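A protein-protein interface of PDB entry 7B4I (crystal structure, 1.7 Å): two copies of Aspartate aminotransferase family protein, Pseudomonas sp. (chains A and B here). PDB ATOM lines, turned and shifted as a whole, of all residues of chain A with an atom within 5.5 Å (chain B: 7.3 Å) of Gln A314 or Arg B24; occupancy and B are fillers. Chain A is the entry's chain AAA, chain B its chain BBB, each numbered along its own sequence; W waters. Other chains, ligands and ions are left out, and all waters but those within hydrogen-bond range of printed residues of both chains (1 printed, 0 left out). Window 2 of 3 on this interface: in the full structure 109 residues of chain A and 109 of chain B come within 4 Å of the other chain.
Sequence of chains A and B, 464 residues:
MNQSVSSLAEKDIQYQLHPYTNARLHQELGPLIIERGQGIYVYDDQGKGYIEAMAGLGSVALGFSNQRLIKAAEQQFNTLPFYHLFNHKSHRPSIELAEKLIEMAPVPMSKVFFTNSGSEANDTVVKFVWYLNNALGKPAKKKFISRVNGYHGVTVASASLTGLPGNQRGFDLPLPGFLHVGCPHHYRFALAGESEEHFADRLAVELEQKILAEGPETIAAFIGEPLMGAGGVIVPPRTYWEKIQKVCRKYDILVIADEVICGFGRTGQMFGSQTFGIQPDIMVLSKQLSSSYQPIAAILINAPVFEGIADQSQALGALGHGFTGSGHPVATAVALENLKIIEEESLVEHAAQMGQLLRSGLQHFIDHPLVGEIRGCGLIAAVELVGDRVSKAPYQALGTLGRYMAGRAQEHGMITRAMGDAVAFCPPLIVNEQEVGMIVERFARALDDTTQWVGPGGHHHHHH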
ATOM      1  N   PHE A 306      29.543  13.721   0.282  1.00  0.00           N
ATOM      2  CA  PHE A 306      29.178  14.614  -0.846  1.00  0.00           C
ATOM      3  C   PHE A 306      28.164  13.907  -1.753  1.00  0.00           C
ATOM      4  O   PHE A 306      27.125  14.497  -2.099  1.00  0.00           O
ATOM      5  CB  PHE A 306      30.382  15.066  -1.668  1.00  0.00           C
ATOM      6  CG  PHE A 306      29.961  15.687  -2.970  1.00  0.00           C
ATOM      7  CD1 PHE A 306      29.285  16.901  -2.979  1.00  0.00           C
ATOM      8  CD2 PHE A 306      30.154  15.022  -4.175  1.00  0.00           C
ATOM      9  CE1 PHE A 306      28.867  17.469  -4.170  1.00  0.00           C
ATOM     10  CE2 PHE A 306      29.731  15.590  -5.365  1.00  0.00           C
ATOM     11  CZ  PHE A 306      29.089  16.813  -5.364  1.00  0.00           C
ATOM     12  N   GLU A 307      28.433  12.652  -2.127  1.00  0.00           N
ATOM     13  CA  GLU A 307      27.596  11.956  -3.147  1.00  0.00           C
ATOM     14  C   GLU A 307      26.156  11.852  -2.617  1.00  0.00           C
ATOM     15  O   GLU A 307      25.225  12.167  -3.378  1.00  0.00           O
ATOM     16  CB  GLU A 307      28.191  10.596  -3.530  1.00  0.00           C
ATOM     17  CG  GLU A 307      29.574  10.684  -4.155  1.00  0.00           C
ATOM     18  CD  GLU A 307      29.680  11.427  -5.479  1.00  0.00           C
ATOM     19  OE1 GLU A 307      28.674  11.492  -6.202  1.00  0.00           O
ATOM     20  OE2 GLU A 307      30.777  11.950  -5.778  1.00  0.00           O
ATOM     21  N   GLY A 308      25.964  11.482  -1.348  1.00  0.00           N
ATOM     22  CA  GLY A 308      24.627  11.409  -0.737  1.00  0.00           C
ATOM     23  C   GLY A 308      23.944  12.770  -0.690  1.00  0.00           C
ATOM     24  O   GLY A 308      22.746  12.865  -1.002  1.00  0.00           O
ATOM     25  N   ILE A 309      24.655  13.799  -0.236  1.00  0.00           N
ATOM     26  CA  ILE A 309      24.082  15.170  -0.141  1.00  0.00           C
ATOM     27  C   ILE A 309      23.715  15.653  -1.547  1.00  0.00           C
ATOM     28  O   ILE A 309      22.620  16.212  -1.715  1.00  0.00           O
ATOM     29  CB  ILE A 309      25.057  16.115   0.586  1.00  0.00           C
ATOM     30  CG1 ILE A 309      25.129  15.758   2.071  1.00  0.00           C
ATOM     31  CG2 ILE A 309      24.657  17.567   0.364  1.00  0.00           C
ATOM     32  CD1 ILE A 309      26.251  16.458   2.820  1.00  0.00           C
ATOM     33  N   ALA A 310      24.600  15.451  -2.514  1.00  0.00           N
ATOM     34  CA  ALA A 310      24.425  15.911  -3.912  1.00  0.00           C
ATOM     35  C   ALA A 310      23.162  15.280  -4.505  1.00  0.00           C
ATOM     36  O   ALA A 310      22.334  16.014  -5.090  1.00  0.00           O
ATOM     37  CB  ALA A 310      25.652  15.570  -4.715  1.00  0.00           C
ATOM     38  N   ASP A 311      22.989  13.971  -4.324  1.00  0.00           N
ATOM     39  CA  ASP A 311      21.791  13.241  -4.823  1.00  0.00           C
ATOM     40  C   ASP A 311      20.535  13.881  -4.232  1.00  0.00           C
ATOM     41  O   ASP A 311      19.626  14.187  -4.989  1.00  0.00           O
ATOM     42  CB  ASP A 311      21.861  11.740  -4.527  1.00  0.00           C
ATOM     43  CG  ASP A 311      22.805  10.977  -5.444  1.00  0.00           C
ATOM     44  OD1 ASP A 311      23.223  11.549  -6.470  1.00  0.00           O
ATOM     45  OD2 ASP A 311      23.143   9.823  -5.108  1.00  0.00           O
ATOM     46  N   GLN A 312      20.497  14.121  -2.926  1.00  0.00           N
ATOM     47  CA  GLN A 312      19.292  14.680  -2.264  1.00  0.00           C
ATOM     48  C   GLN A 312      19.048  16.126  -2.716  1.00  0.00           C
ATOM     49  O   GLN A 312      17.876  16.504  -2.803  1.00  0.00           O
ATOM     50  CB  GLN A 312      19.411  14.599  -0.745  1.00  0.00           C
ATOM     51  CG  GLN A 312      18.106  14.941  -0.049  1.00  0.00           C
ATOM     52  CD  GLN A 312      17.155  13.775  -0.077  1.00  0.00           C
ATOM     53  OE1 GLN A 312      16.943  13.151  -1.115  1.00  0.00           O
ATOM     54  NE2 GLN A 312      16.633  13.435   1.086  1.00  0.00           N
ATOM     55  N   SER A 313      20.092  16.915  -2.976  1.00  0.00           N
ATOM     56  CA  SER A 313      19.947  18.325  -3.430  1.00  0.00           C
ATOM     57  C   SER A 313      19.272  18.343  -4.807  1.00  0.00           C
ATOM     58  O   SER A 313      18.533  19.287  -5.093  1.00  0.00           O
ATOM     59  CB  SER A 313      21.271  19.071  -3.408  1.00  0.00           C
ATOM     60  OG  SER A 313      22.147  18.692  -4.458  1.00  0.00           O
ATOM     61  N   GLN A 314      19.511  17.310  -5.618  1.00  0.00           N
ATOM     62  CA  GLN A 314      18.868  17.128  -6.947  1.00  0.00           C
ATOM     63  C   GLN A 314      17.394  16.772  -6.729  1.00  0.00           C
ATOM     64  O   GLN A 314      16.536  17.459  -7.292  1.00  0.00           O
ATOM     65  CB  GLN A 314      19.632  16.075  -7.754  1.00  0.00           C
ATOM     66  CG  GLN A 314      19.014  15.787  -9.117  1.00  0.00           C
ATOM     67  CD  GLN A 314      19.846  14.790  -9.878  1.00  0.00           C
ATOM     68  OE1 GLN A 314      20.196  13.728  -9.368  1.00  0.00           O
ATOM     69  NE2 GLN A 314      20.213  15.156 -11.089  1.00  0.00           N
ATOM     70  N   ALA A 315      17.110  15.768  -5.898  1.00  0.00           N
ATOM     71  CA  ALA A 315      15.735  15.298  -5.602  1.00  0.00           C
ATOM     72  C   ALA A 315      14.888  16.440  -5.031  1.00  0.00           C
ATOM     73  O   ALA A 315      13.707  16.526  -5.388  1.00  0.00           O
ATOM     74  CB  ALA A 315      15.779  14.127  -4.650  1.00  0.00           C
ATOM     75  N   LEU A 316      15.457  17.281  -4.154  1.00  0.00           N
ATOM     76  CA  LEU A 316      14.708  18.360  -3.452  1.00  0.00           C
ATOM     77  C   LEU A 316      14.865  19.707  -4.162  1.00  0.00           C
ATOM     78  O   LEU A 316      14.385  20.702  -3.592  1.00  0.00           O
ATOM     79  CB  LEU A 316      15.198  18.441  -2.001  1.00  0.00           C
ATOM     80  CG  LEU A 316      15.017  17.160  -1.187  1.00  0.00           C
ATOM     81  CD1 LEU A 316      15.471  17.353   0.248  1.00  0.00           C
ATOM     82  CD2 LEU A 316      13.568  16.699  -1.231  1.00  0.00           C
ATOM     83  N   GLY A 317      15.493  19.755  -5.339  1.00  0.00           N
ATOM     84  CA  GLY A 317      15.510  20.949  -6.206  1.00  0.00           C
ATOM     85  C   GLY A 317      16.790  21.757  -6.048  1.00  0.00           C
ATOM     86  O   GLY A 317      17.364  22.178  -7.063  1.00  0.00           O
ATOM     87  N   ALA A 318      17.198  22.017  -4.808  1.00  0.00           N
ATOM     88  CA  ALA A 318      18.481  22.665  -4.456  1.00  0.00           C
ATOM     89  C   ALA A 318      18.787  22.348  -2.994  1.00  0.00           C
ATOM     90  O   ALA A 318      17.832  22.011  -2.256  1.00  0.00           O
ATOM     91  CB  ALA A 318      18.388  24.149  -4.694  1.00  0.00           C
ATOM     92  N   THR B  21      21.888  25.525  -4.157  1.00  0.00           N
ATOM     93  CA  THR B  21      22.258  25.024  -5.504  1.00  0.00           C
ATOM     94  C   THR B  21      21.958  23.527  -5.567  1.00  0.00           C
ATOM     95  O   THR B  21      22.213  22.832  -4.577  1.00  0.00           O
ATOM     96  CB  THR B  21      23.735  25.307  -5.819  1.00  0.00           C
ATOM     97  OG1 THR B  21      23.961  26.711  -5.733  1.00  0.00           O
ATOM     98  CG2 THR B  21      24.150  24.838  -7.201  1.00  0.00           C
ATOM     99  N   ASN B  22      21.415  23.070  -6.698  1.00  0.00           N
ATOM    100  CA  ASN B  22      21.357  21.625  -7.063  1.00  0.00           C
ATOM    101  C   ASN B  22      22.784  21.169  -7.400  1.00  0.00           C
ATOM    102  O   ASN B  22      23.333  21.623  -8.416  1.00  0.00           O
ATOM    103  CB  ASN B  22      20.348  21.435  -8.199  1.00  0.00           C
ATOM    104  CG  ASN B  22      20.329  20.042  -8.790  1.00  0.00           C
ATOM    105  OD1 ASN B  22      21.281  19.283  -8.642  1.00  0.00           O
ATOM    106  ND2 ASN B  22      19.244  19.711  -9.470  1.00  0.00           N
ATOM    107  N   ALA B  23      23.403  20.354  -6.551  1.00  0.00           N
ATOM    108  CA  ALA B  23      24.832  19.994  -6.653  1.00  0.00           C
ATOM    109  C   ALA B  23      25.092  19.197  -7.949  1.00  0.00           C
ATOM    110  O   ALA B  23      26.207  19.313  -8.512  1.00  0.00           O
ATOM    111  CB  ALA B  23      25.269  19.207  -5.448  1.00  0.00           C
ATOM    112  N   ARG B  24      24.114  18.402  -8.386  1.00  0.00           N
ATOM    113  CA  ARG B  24      24.246  17.567  -9.618  1.00  0.00           C
ATOM    114  C   ARG B  24      24.164  18.471 -10.854  1.00  0.00           C
ATOM    115  O   ARG B  24      25.044  18.351 -11.737  1.00  0.00           O
ATOM    116  CB  ARG B  24      23.186  16.459  -9.623  1.00  0.00           C
ATOM    117  CG  ARG B  24      23.421  15.379  -8.583  1.00  0.00           C
ATOM    118  CD  ARG B  24      24.836  14.841  -8.631  1.00  0.00           C
ATOM    119  NE  ARG B  24      24.952  13.686  -7.760  1.00  0.00           N
ATOM    120  CZ  ARG B  24      26.087  13.157  -7.320  1.00  0.00           C
ATOM    121  NH1 ARG B  24      27.261  13.658  -7.669  1.00  0.00           N
ATOM    122  NH2 ARG B  24      26.035  12.107  -6.521  1.00  0.00           N
ATOM    123  N   LEU B  25      23.167  19.355 -10.907  1.00  0.00           N
ATOM    124  CA  LEU B  25      23.026  20.345 -12.004  1.00  0.00           C
ATOM    125  C   LEU B  25      24.291  21.208 -12.041  1.00  0.00           C
ATOM    126  O   LEU B  25      24.765  21.523 -13.132  1.00  0.00           O
ATOM    127  CB  LEU B  25      21.762  21.180 -11.783  1.00  0.00           C
ATOM    128  CG  LEU B  25      21.434  22.179 -12.889  1.00  0.00           C
ATOM    129  CD1 LEU B  25      21.247  21.465 -14.222  1.00  0.00           C
ATOM    130  CD2 LEU B  25      20.193  22.985 -12.537  1.00  0.00           C
ATOM    131  N   HIS B  26      24.866  21.536 -10.879  1.00  0.00           N
ATOM    132  CA  HIS B  26      26.102  22.348 -10.796  1.00  0.00           C
ATOM    133  C   HIS B  26      27.259  21.620 -11.504  1.00  0.00           C
ATOM    134  O   HIS B  26      28.065  22.297 -12.174  1.00  0.00           O
ATOM    135  CB  HIS B  26      26.434  22.712  -9.342  1.00  0.00           C
ATOM    136  CG  HIS B  26      27.475  23.771  -9.297  1.00  0.00           C
ATOM    137  ND1 HIS B  26      27.226  25.070  -9.691  1.00  0.00           N
ATOM    138  CD2 HIS B  26      28.776  23.710  -8.960  1.00  0.00           C
ATOM    139  CE1 HIS B  26      28.337  25.766  -9.587  1.00  0.00           C
ATOM    140  NE2 HIS B  26      29.301  24.959  -9.134  1.00  0.00           N
ATOM    141  N   GLN B  27      27.367  20.302 -11.336  1.00  0.00           N
ATOM    142  CA  GLN B  27      28.445  19.501 -11.981  1.00  0.00           C
ATOM    143  C   GLN B  27      28.287  19.563 -13.506  1.00  0.00           C
ATOM    144  O   GLN B  27      29.326  19.609 -14.199  1.00  0.00           O
ATOM    145  CB  GLN B  27      28.443  18.074 -11.455  1.00  0.00           C
ATOM    146  CG  GLN B  27      29.018  17.976 -10.059  1.00  0.00           C
ATOM    147  CD  GLN B  27      28.934  16.578  -9.516  1.00  0.00           C
ATOM    148  OE1 GLN B  27      27.874  15.962  -9.503  1.00  0.00           O
ATOM    149  NE2 GLN B  27      30.054  16.100  -9.006  1.00  0.00           N
ATOM    150  N   GLU B  28      27.043  19.637 -13.991  1.00  0.00           N
ATOM    151  CA  GLU B  28      26.703  19.737 -15.432  1.00  0.00           C
ATOM    152  C   GLU B  28      26.941  21.170 -15.932  1.00  0.00           C
ATOM    153  O   GLU B  28      27.733  21.321 -16.863  1.00  0.00           O
ATOM    154  CB  GLU B  28      25.263  19.275 -15.637  1.00  0.00           C
ATOM    155  CG  GLU B  28      24.803  19.228 -17.083  1.00  0.00           C
ATOM    156  CD  GLU B  28      23.291  19.092 -17.233  1.00  0.00           C
ATOM    157  OE1 GLU B  28      22.710  18.198 -16.585  1.00  0.00           O
ATOM    158  OE2 GLU B  28      22.685  19.896 -17.985  1.00  0.00           O
ATOM    159  N   LEU B  29      26.287  22.180 -15.348  1.00  0.00           N
ATOM    160  CA  LEU B  29      26.285  23.575 -15.874  1.00  0.00           C
ATOM    161  C   LEU B  29      27.553  24.324 -15.459  1.00  0.00           C
ATOM    162  O   LEU B  29      27.970  25.223 -16.207  1.00  0.00           O
ATOM    163  CB  LEU B  29      25.053  24.327 -15.360  1.00  0.00           C
ATOM    164  CG  LEU B  29      23.698  23.785 -15.802  1.00  0.00           C
ATOM    165  CD1 LEU B  29      22.579  24.671 -15.277  1.00  0.00           C
ATOM    166  CD2 LEU B  29      23.629  23.663 -17.315  1.00  0.00           C
ATOM    167  N   GLY B  30      28.111  24.027 -14.283  1.00  0.00           N
ATOM    168  CA  GLY B  30      29.217  24.806 -13.697  1.00  0.00           C
ATOM    169  C   GLY B  30      28.743  26.170 -13.194  1.00  0.00           C
ATOM    170  O   GLY B  30      27.555  26.506 -13.270  1.00  0.00           O
HETATM  171  O   HOH W   1      17.110  21.607  -9.650  1.00  0.00           O
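OG of Ser A313 sits at hydrogen-bond distance from N of Ala B23 (3.0 Å).
The guanidinium group of Arg B24 is in salt-bridge range of the side-chain carboxylate of Asp A311.
The side-chain carboxylate (OE1) of Glu A307 lies within salt-bridge range of the guanidinium group (NH2) of Arg B24.
The guanidinium group (NH1) of Arg B24 sits at hydrogen-bond distance from the side-chain amide oxygen (OE1) of Gln B27, at 3.0 Å.
OD1 of Asn B22 lies within hydrogen-bond range of N of Arg B24, at 3.0 Å.
The backbone carbonyl oxygen of Ser A313 lies within hydrogen-bond range of the backbone NH of Ala A318 (3.1 Å).
The side-chain hydroxyl of Ser A313 sits at hydrogen-bond distance from the backbone carbonyl oxygen of Ala A310 (2.8 Å).
OD1 of Asn B22 sits at hydrogen-bond distance from N of Leu B25, 2.9 Å away.
Phe A306 touches Arg B24 (CE2 to NH1, 3.9 Å).
Phe A306 touches Gln B27 (CE2 to NE2, 3.7 Å).
CB of Ala B23 touches CB of Ala A310 (3.7 Å).
Arg B24 touches Ala A310 (CZ to CB, 3.6 Å).
Ser A313 touches Asn B22.
Asn B22 touches Gln A314 (ND2 to CA, 3.6 Å).
Arg B24 touches Gln A314.
O of Gly A317 touches CB of Asn B22, 3.3 Å away.
C of Thr B21 touches CB of Ala A318, at 3.7 Å.
Asn B22 touches Ala A318 (N to CA, 3.7 Å).
Printed residues of chain B within 4 Å of Asp A311: Arg B24 (2.9 Å).
Gln A312 touches none of the printed residues of chain B.
Printed residues of chain B within 4 Å of Ser A313: Asn B22 and Ala B23.
Gln A314 touches two residues of chain B.
Of the printed residues of chain A, Ala B23 touches Ala A310 (3.7 Å) and Ser A313 (3.0 Å).
Arg B24 touches five residues of chain A.
The nearest residue of chain A that does not touch Arg B24 is Ser A313 (4.4 Å).
Hydrophobic or aromatic side chains of chain A within 4 Å of the printed part of chain B: Phe A306, Ala A310 and Ala A318.
Of the 10 printed residues of chain B, 5 touch a printed residue of chain A.
Printed residues of chain B that touch a printed residue of chain A: Thr B21, Asn B22, Ala B23, Arg B24 and Gln B27.
Hydrophobic or aromatic side chains of chain B within 4 Å of the printed part of chain A: Ala B23.
Among the printed residues, 13 pairs touch across the chains.
Among the printed residues, Asp or Glu carboxylates within 4 Å of a Lys or Arg side-chain nitrogen of the other chain: Glu A307 with Arg B24 (2.7 Å) and Asp A311 with Arg B24 (2.9 Å).
No position is printed for both chains.
Water W1 lies within hydrogen-bond range of O of Gly A317 (2.7 Å) and ND2 of Asn B22 (2.9 Å).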
